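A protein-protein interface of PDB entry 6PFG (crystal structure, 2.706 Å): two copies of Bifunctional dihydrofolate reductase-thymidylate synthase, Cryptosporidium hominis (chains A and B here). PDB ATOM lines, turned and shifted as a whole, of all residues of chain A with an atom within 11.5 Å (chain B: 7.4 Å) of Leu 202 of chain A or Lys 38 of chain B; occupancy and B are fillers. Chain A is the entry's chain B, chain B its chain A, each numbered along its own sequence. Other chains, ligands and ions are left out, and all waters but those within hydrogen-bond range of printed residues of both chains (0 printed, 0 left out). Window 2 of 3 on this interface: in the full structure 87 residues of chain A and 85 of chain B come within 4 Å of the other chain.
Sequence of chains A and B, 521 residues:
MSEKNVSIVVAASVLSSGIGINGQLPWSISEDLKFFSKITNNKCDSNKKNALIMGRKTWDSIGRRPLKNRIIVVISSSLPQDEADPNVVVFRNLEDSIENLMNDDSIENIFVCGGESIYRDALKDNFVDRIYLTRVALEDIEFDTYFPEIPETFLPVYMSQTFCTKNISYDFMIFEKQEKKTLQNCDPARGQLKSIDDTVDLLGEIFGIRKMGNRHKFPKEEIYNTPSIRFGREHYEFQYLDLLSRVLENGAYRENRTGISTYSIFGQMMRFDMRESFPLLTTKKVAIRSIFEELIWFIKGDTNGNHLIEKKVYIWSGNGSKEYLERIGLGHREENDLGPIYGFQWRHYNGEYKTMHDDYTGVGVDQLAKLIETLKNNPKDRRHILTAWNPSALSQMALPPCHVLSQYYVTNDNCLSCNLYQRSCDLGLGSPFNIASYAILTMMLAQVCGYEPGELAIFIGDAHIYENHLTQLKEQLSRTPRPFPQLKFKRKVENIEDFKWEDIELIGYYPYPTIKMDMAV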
ATOM      1  N   LYS A 194       4.409 -33.832   8.930  1.00  0.00           N
ATOM      2  CA  LYS A 194       4.550 -34.013  10.371  1.00  0.00           C
ATOM      3  C   LYS A 194       5.856 -33.442  10.910  1.00  0.00           C
ATOM      4  O   LYS A 194       5.944 -33.160  12.109  1.00  0.00           O
ATOM      5  CB  LYS A 194       4.449 -35.498  10.726  1.00  0.00           C
ATOM      6  N   SER A 195       6.874 -33.281  10.060  1.00  0.00           N
ATOM      7  CA  SER A 195       8.160 -32.771  10.531  1.00  0.00           C
ATOM      8  C   SER A 195       8.028 -31.357  11.087  1.00  0.00           C
ATOM      9  O   SER A 195       8.599 -31.040  12.140  1.00  0.00           O
ATOM     10  CB  SER A 195       9.183 -32.806   9.395  1.00  0.00           C
ATOM     11  OG  SER A 195       8.747 -32.032   8.291  1.00  0.00           O
ATOM     12  N   ILE A 196       7.272 -30.498  10.399  1.00  0.00           N
ATOM     13  CA  ILE A 196       7.089 -29.127  10.868  1.00  0.00           C
ATOM     14  C   ILE A 196       6.347 -29.114  12.199  1.00  0.00           C
ATOM     15  O   ILE A 196       6.725 -28.392  13.131  1.00  0.00           O
ATOM     16  CB  ILE A 196       6.362 -28.290   9.800  1.00  0.00           C
ATOM     17  CG1 ILE A 196       7.192 -28.229   8.518  1.00  0.00           C
ATOM     18  CG2 ILE A 196       6.076 -26.886  10.319  1.00  0.00           C
ATOM     19  CD1 ILE A 196       6.542 -27.430   7.411  1.00  0.00           C
ATOM     20  N   ASP A 197       5.283 -29.913  12.309  1.00  0.00           N
ATOM     21  CA  ASP A 197       4.521 -29.962  13.554  1.00  0.00           C
ATOM     22  C   ASP A 197       5.380 -30.466  14.707  1.00  0.00           C
ATOM     23  O   ASP A 197       5.316 -29.929  15.819  1.00  0.00           O
ATOM     24  CB  ASP A 197       3.285 -30.845  13.378  1.00  0.00           C
ATOM     25  CG  ASP A 197       2.334 -30.315  12.320  1.00  0.00           C
ATOM     26  OD1 ASP A 197       2.757 -29.466  11.506  1.00  0.00           O
ATOM     27  OD2 ASP A 197       1.162 -30.748  12.301  1.00  0.00           O
ATOM     28  N   ASP A 198       6.201 -31.490  14.457  1.00  0.00           N
ATOM     29  CA  ASP A 198       7.069 -32.013  15.508  1.00  0.00           C
ATOM     30  C   ASP A 198       8.113 -30.988  15.930  1.00  0.00           C
ATOM     31  O   ASP A 198       8.372 -30.819  17.128  1.00  0.00           O
ATOM     32  CB  ASP A 198       7.746 -33.305  15.045  1.00  0.00           C
ATOM     33  CG  ASP A 198       6.776 -34.463  14.924  1.00  0.00           C
ATOM     34  OD1 ASP A 198       5.663 -34.373  15.485  1.00  0.00           O
ATOM     35  OD2 ASP A 198       7.131 -35.470  14.278  1.00  0.00           O
ATOM     36  N   THR A 199       8.721 -30.289  14.967  1.00  0.00           N
ATOM     37  CA  THR A 199       9.708 -29.273  15.318  1.00  0.00           C
ATOM     38  C   THR A 199       9.074 -28.139  16.117  1.00  0.00           C
ATOM     39  O   THR A 199       9.663 -27.652  17.092  1.00  0.00           O
ATOM     40  CB  THR A 199      10.383 -28.738  14.054  1.00  0.00           C
ATOM     41  OG1 THR A 199      11.069 -29.806  13.389  1.00  0.00           O
ATOM     42  CG2 THR A 199      11.383 -27.651  14.401  1.00  0.00           C
ATOM     43  N   VAL A 200       7.873 -27.707  15.723  1.00  0.00           N
ATOM     44  CA  VAL A 200       7.189 -26.645  16.457  1.00  0.00           C
ATOM     45  C   VAL A 200       6.842 -27.105  17.869  1.00  0.00           C
ATOM     46  O   VAL A 200       6.981 -26.343  18.834  1.00  0.00           O
ATOM     47  CB  VAL A 200       5.944 -26.174  15.680  1.00  0.00           C
ATOM     48  CG1 VAL A 200       5.092 -25.244  16.533  1.00  0.00           C
ATOM     49  CG2 VAL A 200       6.366 -25.464  14.411  1.00  0.00           C
ATOM     50  N   ASP A 201       6.399 -28.357  18.018  1.00  0.00           N
ATOM     51  CA  ASP A 201       6.093 -28.871  19.350  1.00  0.00           C
ATOM     52  C   ASP A 201       7.344 -28.937  20.218  1.00  0.00           C
ATOM     53  O   ASP A 201       7.302 -28.612  21.411  1.00  0.00           O
ATOM     54  CB  ASP A 201       5.439 -30.250  19.251  1.00  0.00           C
ATOM     55  CG  ASP A 201       4.035 -30.189  18.685  1.00  0.00           C
ATOM     56  OD1 ASP A 201       3.371 -29.146  18.853  1.00  0.00           O
ATOM     57  OD2 ASP A 201       3.594 -31.186  18.076  1.00  0.00           O
ATOM     58  N   LEU A 202       8.471 -29.351  19.636  1.00  0.00           N
ATOM     59  CA  LEU A 202       9.711 -29.404  20.403  1.00  0.00           C
ATOM     60  C   LEU A 202      10.165 -28.008  20.815  1.00  0.00           C
ATOM     61  O   LEU A 202      10.620 -27.807  21.950  1.00  0.00           O
ATOM     62  CB  LEU A 202      10.797 -30.110  19.593  1.00  0.00           C
ATOM     63  CG  LEU A 202      10.550 -31.595  19.311  1.00  0.00           C
ATOM     64  CD1 LEU A 202      11.678 -32.176  18.476  1.00  0.00           C
ATOM     65  CD2 LEU A 202      10.367 -32.382  20.601  1.00  0.00           C
ATOM     66  N   LEU A 203      10.051 -27.032  19.911  1.00  0.00           N
ATOM     67  CA  LEU A 203      10.406 -25.660  20.264  1.00  0.00           C
ATOM     68  C   LEU A 203       9.486 -25.110  21.349  1.00  0.00           C
ATOM     69  O   LEU A 203       9.925 -24.349  22.218  1.00  0.00           O
ATOM     70  CB  LEU A 203      10.379 -24.769  19.025  1.00  0.00           C
ATOM     71  CG  LEU A 203      11.523 -24.988  18.038  1.00  0.00           C
ATOM     72  CD1 LEU A 203      11.363 -24.085  16.824  1.00  0.00           C
ATOM     73  CD2 LEU A 203      12.859 -24.747  18.718  1.00  0.00           C
ATOM     74  N   GLY A 204       8.204 -25.482  21.314  1.00  0.00           N
ATOM     75  CA  GLY A 204       7.291 -25.072  22.367  1.00  0.00           C
ATOM     76  C   GLY A 204       7.510 -25.792  23.682  1.00  0.00           C
ATOM     77  O   GLY A 204       7.077 -25.298  24.727  1.00  0.00           O
ATOM     78  N   GLU A 205       8.142 -26.963  23.649  1.00  0.00           N
ATOM     79  CA  GLU A 205       8.539 -27.617  24.891  1.00  0.00           C
ATOM     80  C   GLU A 205       9.792 -26.974  25.474  1.00  0.00           C
ATOM     81  O   GLU A 205       9.889 -26.788  26.692  1.00  0.00           O
ATOM     82  CB  GLU A 205       8.764 -29.110  24.661  1.00  0.00           C
ATOM     83  CG  GLU A 205       7.492 -29.887  24.386  1.00  0.00           C
ATOM     84  CD  GLU A 205       7.756 -31.348  24.089  1.00  0.00           C
ATOM     85  OE1 GLU A 205       8.925 -31.777  24.199  1.00  0.00           O
ATOM     86  OE2 GLU A 205       6.794 -32.067  23.745  1.00  0.00           O
ATOM     87  N   ILE A 206      10.754 -26.628  24.622  1.00  0.00           N
ATOM     88  CA  ILE A 206      11.977 -25.972  25.073  1.00  0.00           C
ATOM     89  C   ILE A 206      11.644 -24.596  25.632  1.00  0.00           C
ATOM     90  O   ILE A 206      11.764 -24.361  26.838  1.00  0.00           O
ATOM     91  CB  ILE A 206      13.005 -25.874  23.935  1.00  0.00           C
ATOM     92  CG1 ILE A 206      13.425 -27.271  23.487  1.00  0.00           C
ATOM     93  CG2 ILE A 206      14.212 -25.056  24.374  1.00  0.00           C
ATOM     94  CD1 ILE A 206      14.203 -27.273  22.211  1.00  0.00           C
ATOM     95  N   PHE A 207      11.231 -23.675  24.765  1.00  0.00           N
ATOM     96  CA  PHE A 207      10.800 -22.359  25.215  1.00  0.00           C
ATOM     97  C   PHE A 207       9.381 -22.436  25.754  1.00  0.00           C
ATOM     98  O   PHE A 207       8.519 -23.102  25.178  1.00  0.00           O
ATOM     99  CB  PHE A 207      10.864 -21.343  24.078  1.00  0.00           C
ATOM    100  CG  PHE A 207      12.195 -21.275  23.397  1.00  0.00           C
ATOM    101  CD1 PHE A 207      13.181 -20.425  23.868  1.00  0.00           C
ATOM    102  CD2 PHE A 207      12.458 -22.046  22.279  1.00  0.00           C
ATOM    103  CE1 PHE A 207      14.407 -20.351  23.240  1.00  0.00           C
ATOM    104  CE2 PHE A 207      13.680 -21.976  21.647  1.00  0.00           C
ATOM    105  CZ  PHE A 207      14.657 -21.127  22.128  1.00  0.00           C
ATOM    106  N   GLY A 208       9.137 -21.751  26.861  1.00  0.00           N
ATOM    107  CA  GLY A 208       7.818 -21.799  27.455  1.00  0.00           C
ATOM    108  C   GLY A 208       6.874 -20.819  26.802  1.00  0.00           C
ATOM    109  O   GLY A 208       6.538 -20.955  25.621  1.00  0.00           O
ATOM    110  N   ILE A 209       6.437 -19.824  27.569  1.00  0.00           N
ATOM    111  CA  ILE A 209       5.693 -18.701  27.015  1.00  0.00           C
ATOM    112  C   ILE A 209       6.657 -17.772  26.291  1.00  0.00           C
ATOM    113  O   ILE A 209       6.248 -16.734  25.760  1.00  0.00           O
ATOM    114  CB  ILE A 209       4.913 -17.960  28.114  1.00  0.00           C
ATOM    115  CG1 ILE A 209       5.861 -17.493  29.220  1.00  0.00           C
ATOM    116  CG2 ILE A 209       3.840 -18.864  28.696  1.00  0.00           C
ATOM    117  CD1 ILE A 209       5.171 -16.779  30.366  1.00  0.00           C
ATOM    118  N   ARG A 210       7.947 -18.132  26.270  1.00  0.00           N
ATOM    119  CA  ARG A 210       8.910 -17.376  25.476  1.00  0.00           C
ATOM    120  C   ARG A 210       8.624 -17.492  23.983  1.00  0.00           C
ATOM    121  O   ARG A 210       8.942 -16.573  23.220  1.00  0.00           O
ATOM    122  CB  ARG A 210      10.335 -17.841  25.779  1.00  0.00           C
ATOM    123  CG  ARG A 210      10.785 -17.600  27.210  1.00  0.00           C
ATOM    124  CD  ARG A 210      12.172 -18.168  27.441  1.00  0.00           C
ATOM    125  NE  ARG A 210      13.130 -17.680  26.454  1.00  0.00           N
ATOM    126  CZ  ARG A 210      14.360 -18.160  26.317  1.00  0.00           C
ATOM    127  NH1 ARG A 210      14.774 -19.145  27.100  1.00  0.00           N
ATOM    128  NH2 ARG A 210      15.175 -17.664  25.396  1.00  0.00           N
ATOM    129  N   LYS A 211       8.028 -18.601  23.548  1.00  0.00           N
ATOM    130  CA  LYS A 211       7.618 -18.778  22.160  1.00  0.00           C
ATOM    131  C   LYS A 211       6.195 -18.256  21.994  1.00  0.00           C
ATOM    132  O   LYS A 211       5.263 -18.770  22.624  1.00  0.00           O
ATOM    133  CB  LYS A 211       7.714 -20.249  21.756  1.00  0.00           C
ATOM    134  CG  LYS A 211       7.163 -20.569  20.379  1.00  0.00           C
ATOM    135  CD  LYS A 211       7.655 -21.928  19.902  1.00  0.00           C
ATOM    136  CE  LYS A 211       6.757 -22.502  18.819  1.00  0.00           C
ATOM    137  NZ  LYS A 211       6.469 -21.518  17.741  1.00  0.00           N
ATOM    138  N   GLY A 213       3.881 -18.527  19.918  1.00  0.00           N
ATOM    139  CA  GLY A 213       2.834 -19.479  19.587  1.00  0.00           C
ATOM    140  C   GLY A 213       2.175 -20.093  20.807  1.00  0.00           C
ATOM    141  O   GLY A 213       0.970 -20.364  20.794  1.00  0.00           O
ATOM    142  N   ASN A 214       2.944 -20.315  21.877  1.00  0.00           N
ATOM    143  CA  ASN A 214       2.372 -20.851  23.107  1.00  0.00           C
ATOM    144  C   ASN A 214       1.466 -19.847  23.808  1.00  0.00           C
ATOM    145  O   ASN A 214       0.655 -20.246  24.649  1.00  0.00           O
ATOM    146  CB  ASN A 214       3.481 -21.307  24.055  1.00  0.00           C
ATOM    147  CG  ASN A 214       4.034 -22.669  23.691  1.00  0.00           C
ATOM    148  OD1 ASN A 214       3.314 -23.524  23.176  1.00  0.00           O
ATOM    149  ND2 ASN A 214       5.318 -22.879  23.957  1.00  0.00           N
ATOM    150  N   ASP B  32      19.832 -24.256  22.102  1.00  0.00           N
ATOM    151  CA  ASP B  32      20.220 -24.946  20.875  1.00  0.00           C
ATOM    152  C   ASP B  32      20.659 -26.379  21.162  1.00  0.00           C
ATOM    153  O   ASP B  32      20.346 -27.295  20.391  1.00  0.00           O
ATOM    154  CB  ASP B  32      21.327 -24.171  20.165  1.00  0.00           C
ATOM    155  CG  ASP B  32      21.887 -24.919  18.976  1.00  0.00           C
ATOM    156  OD1 ASP B  32      21.119 -25.197  18.030  1.00  0.00           O
ATOM    157  OD2 ASP B  32      23.097 -25.224  18.987  1.00  0.00           O
ATOM    158  N   LEU B  33      21.373 -26.596  22.271  1.00  0.00           N
ATOM    159  CA  LEU B  33      21.709 -27.961  22.665  1.00  0.00           C
ATOM    160  C   LEU B  33      20.460 -28.752  23.030  1.00  0.00           C
ATOM    161  O   LEU B  33      20.358 -29.944  22.711  1.00  0.00           O
ATOM    162  CB  LEU B  33      22.695 -27.955  23.834  1.00  0.00           C
ATOM    163  CG  LEU B  33      24.091 -27.396  23.559  1.00  0.00           C
ATOM    164  CD1 LEU B  33      24.977 -27.554  24.787  1.00  0.00           C
ATOM    165  CD2 LEU B  33      24.710 -28.080  22.347  1.00  0.00           C
ATOM    166  N   LYS B  34      19.500 -28.112  23.703  1.00  0.00           N
ATOM    167  CA  LYS B  34      18.248 -28.795  24.013  1.00  0.00           C
ATOM    168  C   LYS B  34      17.495 -29.160  22.739  1.00  0.00           C
ATOM    169  O   LYS B  34      16.879 -30.231  22.656  1.00  0.00           O
ATOM    170  CB  LYS B  34      17.382 -27.924  24.925  1.00  0.00           C
ATOM    171  CG  LYS B  34      18.035 -27.614  26.267  1.00  0.00           C
ATOM    172  CD  LYS B  34      17.064 -26.957  27.232  1.00  0.00           C
ATOM    173  CE  LYS B  34      17.755 -26.587  28.537  1.00  0.00           C
ATOM    174  NZ  LYS B  34      18.413 -27.762  29.175  1.00  0.00           N
ATOM    175  N   PHE B  35      17.542 -28.286  21.731  1.00  0.00           N
ATOM    176  CA  PHE B  35      16.925 -28.596  20.447  1.00  0.00           C
ATOM    177  C   PHE B  35      17.613 -29.783  19.790  1.00  0.00           C
ATOM    178  O   PHE B  35      16.952 -30.689  19.273  1.00  0.00           O
ATOM    179  CB  PHE B  35      16.968 -27.371  19.532  1.00  0.00           C
ATOM    180  CG  PHE B  35      16.410 -27.620  18.159  1.00  0.00           C
ATOM    181  CD1 PHE B  35      15.041 -27.673  17.952  1.00  0.00           C
ATOM    182  CD2 PHE B  35      17.254 -27.790  17.074  1.00  0.00           C
ATOM    183  CE1 PHE B  35      14.522 -27.899  16.687  1.00  0.00           C
ATOM    184  CE2 PHE B  35      16.742 -28.014  15.806  1.00  0.00           C
ATOM    185  CZ  PHE B  35      15.374 -28.069  15.614  1.00  0.00           C
ATOM    186  N   PHE B  36      18.948 -29.785  19.790  1.00  0.00           N
ATOM    187  CA  PHE B  36      19.693 -30.926  19.266  1.00  0.00           C
ATOM    188  C   PHE B  36      19.261 -32.215  19.952  1.00  0.00           C
ATOM    189  O   PHE B  36      18.979 -33.223  19.294  1.00  0.00           O
ATOM    190  CB  PHE B  36      21.196 -30.693  19.449  1.00  0.00           C
ATOM    191  CG  PHE B  36      22.052 -31.852  19.012  1.00  0.00           C
ATOM    192  CD1 PHE B  36      22.530 -31.924  17.714  1.00  0.00           C
ATOM    193  CD2 PHE B  36      22.388 -32.862  19.900  1.00  0.00           C
ATOM    194  CE1 PHE B  36      23.319 -32.983  17.308  1.00  0.00           C
ATOM    195  CE2 PHE B  36      23.171 -33.924  19.500  1.00  0.00           C
ATOM    196  CZ  PHE B  36      23.640 -33.985  18.203  1.00  0.00           C
ATOM    197  N   SER B  37      19.195 -32.190  21.285  1.00  0.00           N
ATOM    198  CA  SER B  37      18.823 -33.383  22.040  1.00  0.00           C
ATOM    199  C   SER B  37      17.421 -33.856  21.677  1.00  0.00           C
ATOM    200  O   SER B  37      17.206 -35.042  21.401  1.00  0.00           O
ATOM    201  CB  SER B  37      18.926 -33.103  23.539  1.00  0.00           C
ATOM    202  OG  SER B  37      18.508 -34.229  24.291  1.00  0.00           O
ATOM    203  N   LYS B  38      16.450 -32.939  21.667  1.00  0.00           N
ATOM    204  CA  LYS B  38      15.071 -33.343  21.412  1.00  0.00           C
ATOM    205  C   LYS B  38      14.863 -33.790  19.972  1.00  0.00           C
ATOM    206  O   LYS B  38      14.027 -34.661  19.712  1.00  0.00           O
ATOM    207  CB  LYS B  38      14.107 -32.209  21.761  1.00  0.00           C
ATOM    208  CG  LYS B  38      14.108 -31.854  23.233  1.00  0.00           C
ATOM    209  CD  LYS B  38      12.779 -31.272  23.672  1.00  0.00           C
ATOM    210  CE  LYS B  38      12.703 -31.206  25.188  1.00  0.00           C
ATOM    211  NZ  LYS B  38      11.348 -30.827  25.666  1.00  0.00           N
ATOM    212  N   ILE B  39      15.610 -33.222  19.026  1.00  0.00           N
ATOM    213  CA  ILE B  39      15.413 -33.604  17.634  1.00  0.00           C
ATOM    214  C   ILE B  39      16.140 -34.908  17.322  1.00  0.00           C
ATOM    215  O   ILE B  39      15.701 -35.669  16.452  1.00  0.00           O
ATOM    216  CB  ILE B  39      15.846 -32.461  16.696  1.00  0.00           C
ATOM    217  CG1 ILE B  39      15.168 -32.603  15.334  1.00  0.00           C
ATOM    218  CG2 ILE B  39      17.355 -32.425  16.523  1.00  0.00           C
ATOM    219  CD1 ILE B  39      13.670 -32.403  15.383  1.00  0.00           C
ATOM    220  N   THR B  40      17.237 -35.208  18.027  1.00  0.00           N
ATOM    221  CA  THR B  40      17.934 -36.468  17.806  1.00  0.00           C
ATOM    222  C   THR B  40      17.334 -37.618  18.604  1.00  0.00           C
ATOM    223  O   THR B  40      17.528 -38.778  18.227  1.00  0.00           O
ATOM    224  CB  THR B  40      19.419 -36.323  18.148  1.00  0.00           C
ATOM    225  OG1 THR B  40      19.559 -35.834  19.488  1.00  0.00           O
ATOM    226  CG2 THR B  40      20.099 -35.360  17.183  1.00  0.00           C
ATOM    227  N   ASN B  41      16.619 -37.327  19.689  1.00  0.00           N
ATOM    228  CA  ASN B  41      15.904 -38.347  20.444  1.00  0.00           C
ATOM    229  C   ASN B  41      14.506 -38.617  19.904  1.00  0.00           C
ATOM    230  O   ASN B  41      13.897 -39.623  20.283  1.00  0.00           O
ATOM    231  CB  ASN B  41      15.807 -37.943  21.918  1.00  0.00           C
ATOM    232  CG  ASN B  41      17.045 -38.313  22.707  1.00  0.00           C
ATOM    233  OD1 ASN B  41      17.517 -39.449  22.648  1.00  0.00           O
ATOM    234  ND2 ASN B  41      17.586 -37.351  23.443  1.00  0.00           N
ATOM    235  N   ASN B  42      13.984 -37.742  19.046  1.00  0.00           N
ATOM    236  CA  ASN B  42      12.638 -37.889  18.507  1.00  0.00           C
ATOM    237  C   ASN B  42      12.523 -39.157  17.668  1.00  0.00           C
ATOM    238  O   ASN B  42      13.116 -39.253  16.590  1.00  0.00           O
ATOM    239  CB  ASN B  42      12.270 -36.659  17.672  1.00  0.00           C
ATOM    240  CG  ASN B  42      10.809 -36.640  17.275  1.00  0.00           C
ATOM    241  OD1 ASN B  42       9.948 -37.120  18.010  1.00  0.00           O
ATOM    242  ND2 ASN B  42      10.523 -36.086  16.101  1.00  0.00           N
ATOM    243  N   LYS B  43      11.765 -40.137  18.157  1.00  0.00           N
ATOM    244  CA  LYS B  43      11.590 -41.400  17.458  1.00  0.00           C
ATOM    245  C   LYS B  43      10.173 -41.905  17.684  1.00  0.00           C
ATOM    246  O   LYS B  43       9.467 -41.454  18.589  1.00  0.00           O
ATOM    247  CB  LYS B  43      12.604 -42.454  17.923  1.00  0.00           C
ATOM    248  CG  LYS B  43      12.477 -42.825  19.390  1.00  0.00           C
ATOM    249  CD  LYS B  43      13.492 -43.882  19.785  1.00  0.00           C
ATOM    250  CE  LYS B  43      13.250 -44.362  21.202  1.00  0.00           C
ATOM    251  NZ  LYS B  43      14.190 -45.448  21.591  1.00  0.00           N
ATOM    252  N   ASN B  50      18.094 -44.038  17.530  1.00  0.00           N
ATOM    253  CA  ASN B  50      18.545 -43.197  16.433  1.00  0.00           C
ATOM    254  C   ASN B  50      20.069 -43.184  16.383  1.00  0.00           C
ATOM    255  O   ASN B  50      20.745 -43.309  17.407  1.00  0.00           O
ATOM    256  CB  ASN B  50      18.008 -41.770  16.572  1.00  0.00           C
ATOM    257  CG  ASN B  50      16.513 -41.680  16.312  1.00  0.00           C
ATOM    258  OD1 ASN B  50      15.955 -42.467  15.547  1.00  0.00           O
ATOM    259  ND2 ASN B  50      15.861 -40.709  16.940  1.00  0.00           N
ATOM    260  N   ARG B  70      20.880 -42.772  22.603  1.00  0.00           N
ATOM    261  CA  ARG B  70      21.210 -42.766  21.186  1.00  0.00           C
ATOM    262  C   ARG B  70      22.506 -43.530  20.944  1.00  0.00           C
ATOM    263  O   ARG B  70      23.270 -43.826  21.867  1.00  0.00           O
ATOM    264  CB  ARG B  70      21.327 -41.332  20.657  1.00  0.00           C
ATOM    265  CG  ARG B  70      19.999 -40.602  20.549  1.00  0.00           C
ATOM    266  CD  ARG B  70      20.179 -39.110  20.766  1.00  0.00           C
ATOM    267  NE  ARG B  70      20.562 -38.810  22.142  1.00  0.00           N
ATOM    268  CZ  ARG B  70      20.890 -37.600  22.578  1.00  0.00           C
ATOM    269  NH1 ARG B  70      20.889 -36.570  21.744  1.00  0.00           N
ATOM    270  NH2 ARG B  70      21.223 -37.420  23.850  1.00  0.00           N
ATOM    271  N   PHE B 111      21.085 -39.184  11.706  1.00  0.00           N
ATOM    272  CA  PHE B 111      21.397 -37.764  11.801  1.00  0.00           C
ATOM    273  C   PHE B 111      22.879 -37.539  11.540  1.00  0.00           C
ATOM    274  O   PHE B 111      23.729 -38.160  12.185  1.00  0.00           O
ATOM    275  CB  PHE B 111      21.016 -37.204  13.176  1.00  0.00           C
ATOM    276  CG  PHE B 111      19.544 -37.239  13.458  1.00  0.00           C
ATOM    277  CD1 PHE B 111      18.980 -38.307  14.136  1.00  0.00           C
ATOM    278  CD2 PHE B 111      18.722 -36.203  13.042  1.00  0.00           C
ATOM    279  CE1 PHE B 111      17.622 -38.341  14.397  1.00  0.00           C
ATOM    280  CE2 PHE B 111      17.362 -36.231  13.299  1.00  0.00           C
ATOM    281  CZ  PHE B 111      16.811 -37.302  13.977  1.00  0.00           C
ATOM    282  N   TYR B 132      18.094 -29.553   9.521  1.00  0.00           N
ATOM    283  CA  TYR B 132      17.692 -28.717  10.646  1.00  0.00           C
ATOM    284  C   TYR B 132      18.818 -27.726  10.922  1.00  0.00           C
ATOM    285  O   TYR B 132      19.869 -28.102  11.462  1.00  0.00           O
ATOM    286  CB  TYR B 132      17.392 -29.562  11.883  1.00  0.00           C
ATOM    287  CG  TYR B 132      16.214 -30.505  11.745  1.00  0.00           C
ATOM    288  CD1 TYR B 132      14.924 -30.081  12.041  1.00  0.00           C
ATOM    289  CD2 TYR B 132      16.394 -31.823  11.349  1.00  0.00           C
ATOM    290  CE1 TYR B 132      13.844 -30.937  11.929  1.00  0.00           C
ATOM    291  CE2 TYR B 132      15.319 -32.689  11.237  1.00  0.00           C
ATOM    292  CZ  TYR B 132      14.047 -32.240  11.528  1.00  0.00           C
ATOM    293  OH  TYR B 132      12.973 -33.095  11.419  1.00  0.00           O
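The backbone carbonyl oxygen of Asn 42 of chain B is in hydrogen-bond range of the side-chain amide nitrogen of Asn 50 of chain B (3.1 Å).
The backbone carbonyl oxygen (O) of Ser 195 of chain A is in hydrogen-bond range of the side-chain hydroxyl (OG1) of Thr 199 of chain A.
No position is printed for both chains.
Hydrophobic or aromatic side chains of chain A that line the printed part of chain B: Leu 202, Leu 203 and Ile 206.
Hydrophobic or aromatic side chains of chain B within 4 Å of the printed part of chain A: Phe 35, Ile 39 and Tyr 132.
Among the printed residues, 9 pairs touch across the chains.
Among the printed residues, Asp or Glu carboxylates within 4 Å of a Lys or Arg side-chain nitrogen of the other chain: Glu 205 of chain A with Lys 38 of chain B (3.0 Å).
Of the printed residues of chain B, Leu 203 of chain A touches Phe 35 (3.7 Å).
Of the printed residues of chain B, Ile 206 of chain A touches Lys 34 (3.8 Å) and Phe 35 (3.5 Å).
Of the printed residues of chain A, Lys 34 of chain B touches Ile 206 (3.8 Å).
Phe 35 of chain B touches just these residues of chain A: Thr 199 (3.9 Å), Leu 203 (3.7 Å) and Ile 206 (3.5 Å).
Lys 38 of chain B touches two residues of chain A.
Of chain A, only Leu 202 comes within 4 Å of Ile 39 of chain B.
No residue of chain A comes within 4 Å of Thr 40 of chain B.
No residue of chain A comes within 4 Å of Asn 41 of chain B.
Of chain A, only Asp 198 comes within 4 Å of Asn 42 of chain B.
Printed residues of chain A within 4 Å of Tyr 132 of chain B: Thr 199.
The nearest residue of chain A that does not touch Lys 38 of chain B is Ile 206 of chain A (4.1 Å).
The side-chain carboxylate (OE1) of Glu 205 of chain A lies within salt-bridge range of the side-chain amino group (NZ) of Lys 38 of chain B, 3.0 Å away.
Asn 42 of chain B touches Asp 198 of chain A (ND2 to OD2, 3.9 Å).
Phe 35 of chain B touches Thr 199 of chain A (CE1 to CG2, 3.9 Å).
Tyr 132 of chain B touches Thr 199 of chain A (CE1 to OG1, 3.3 Å).
O of Lys 38 of chain B touches CD1 of Leu 202 of chain A, at 3.6 Å.
Leu 202 of chain A touches Ile 39 of chain B.
Leu 203 of chain A touches Phe 35 of chain B.
Lys 34 of chain B touches Ile 206 of chain A (C to CD1, 3.8 Å).
CD1 of Ile 206 of chain A touches CA of Phe 35 of chain B, 3.5 Å away.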
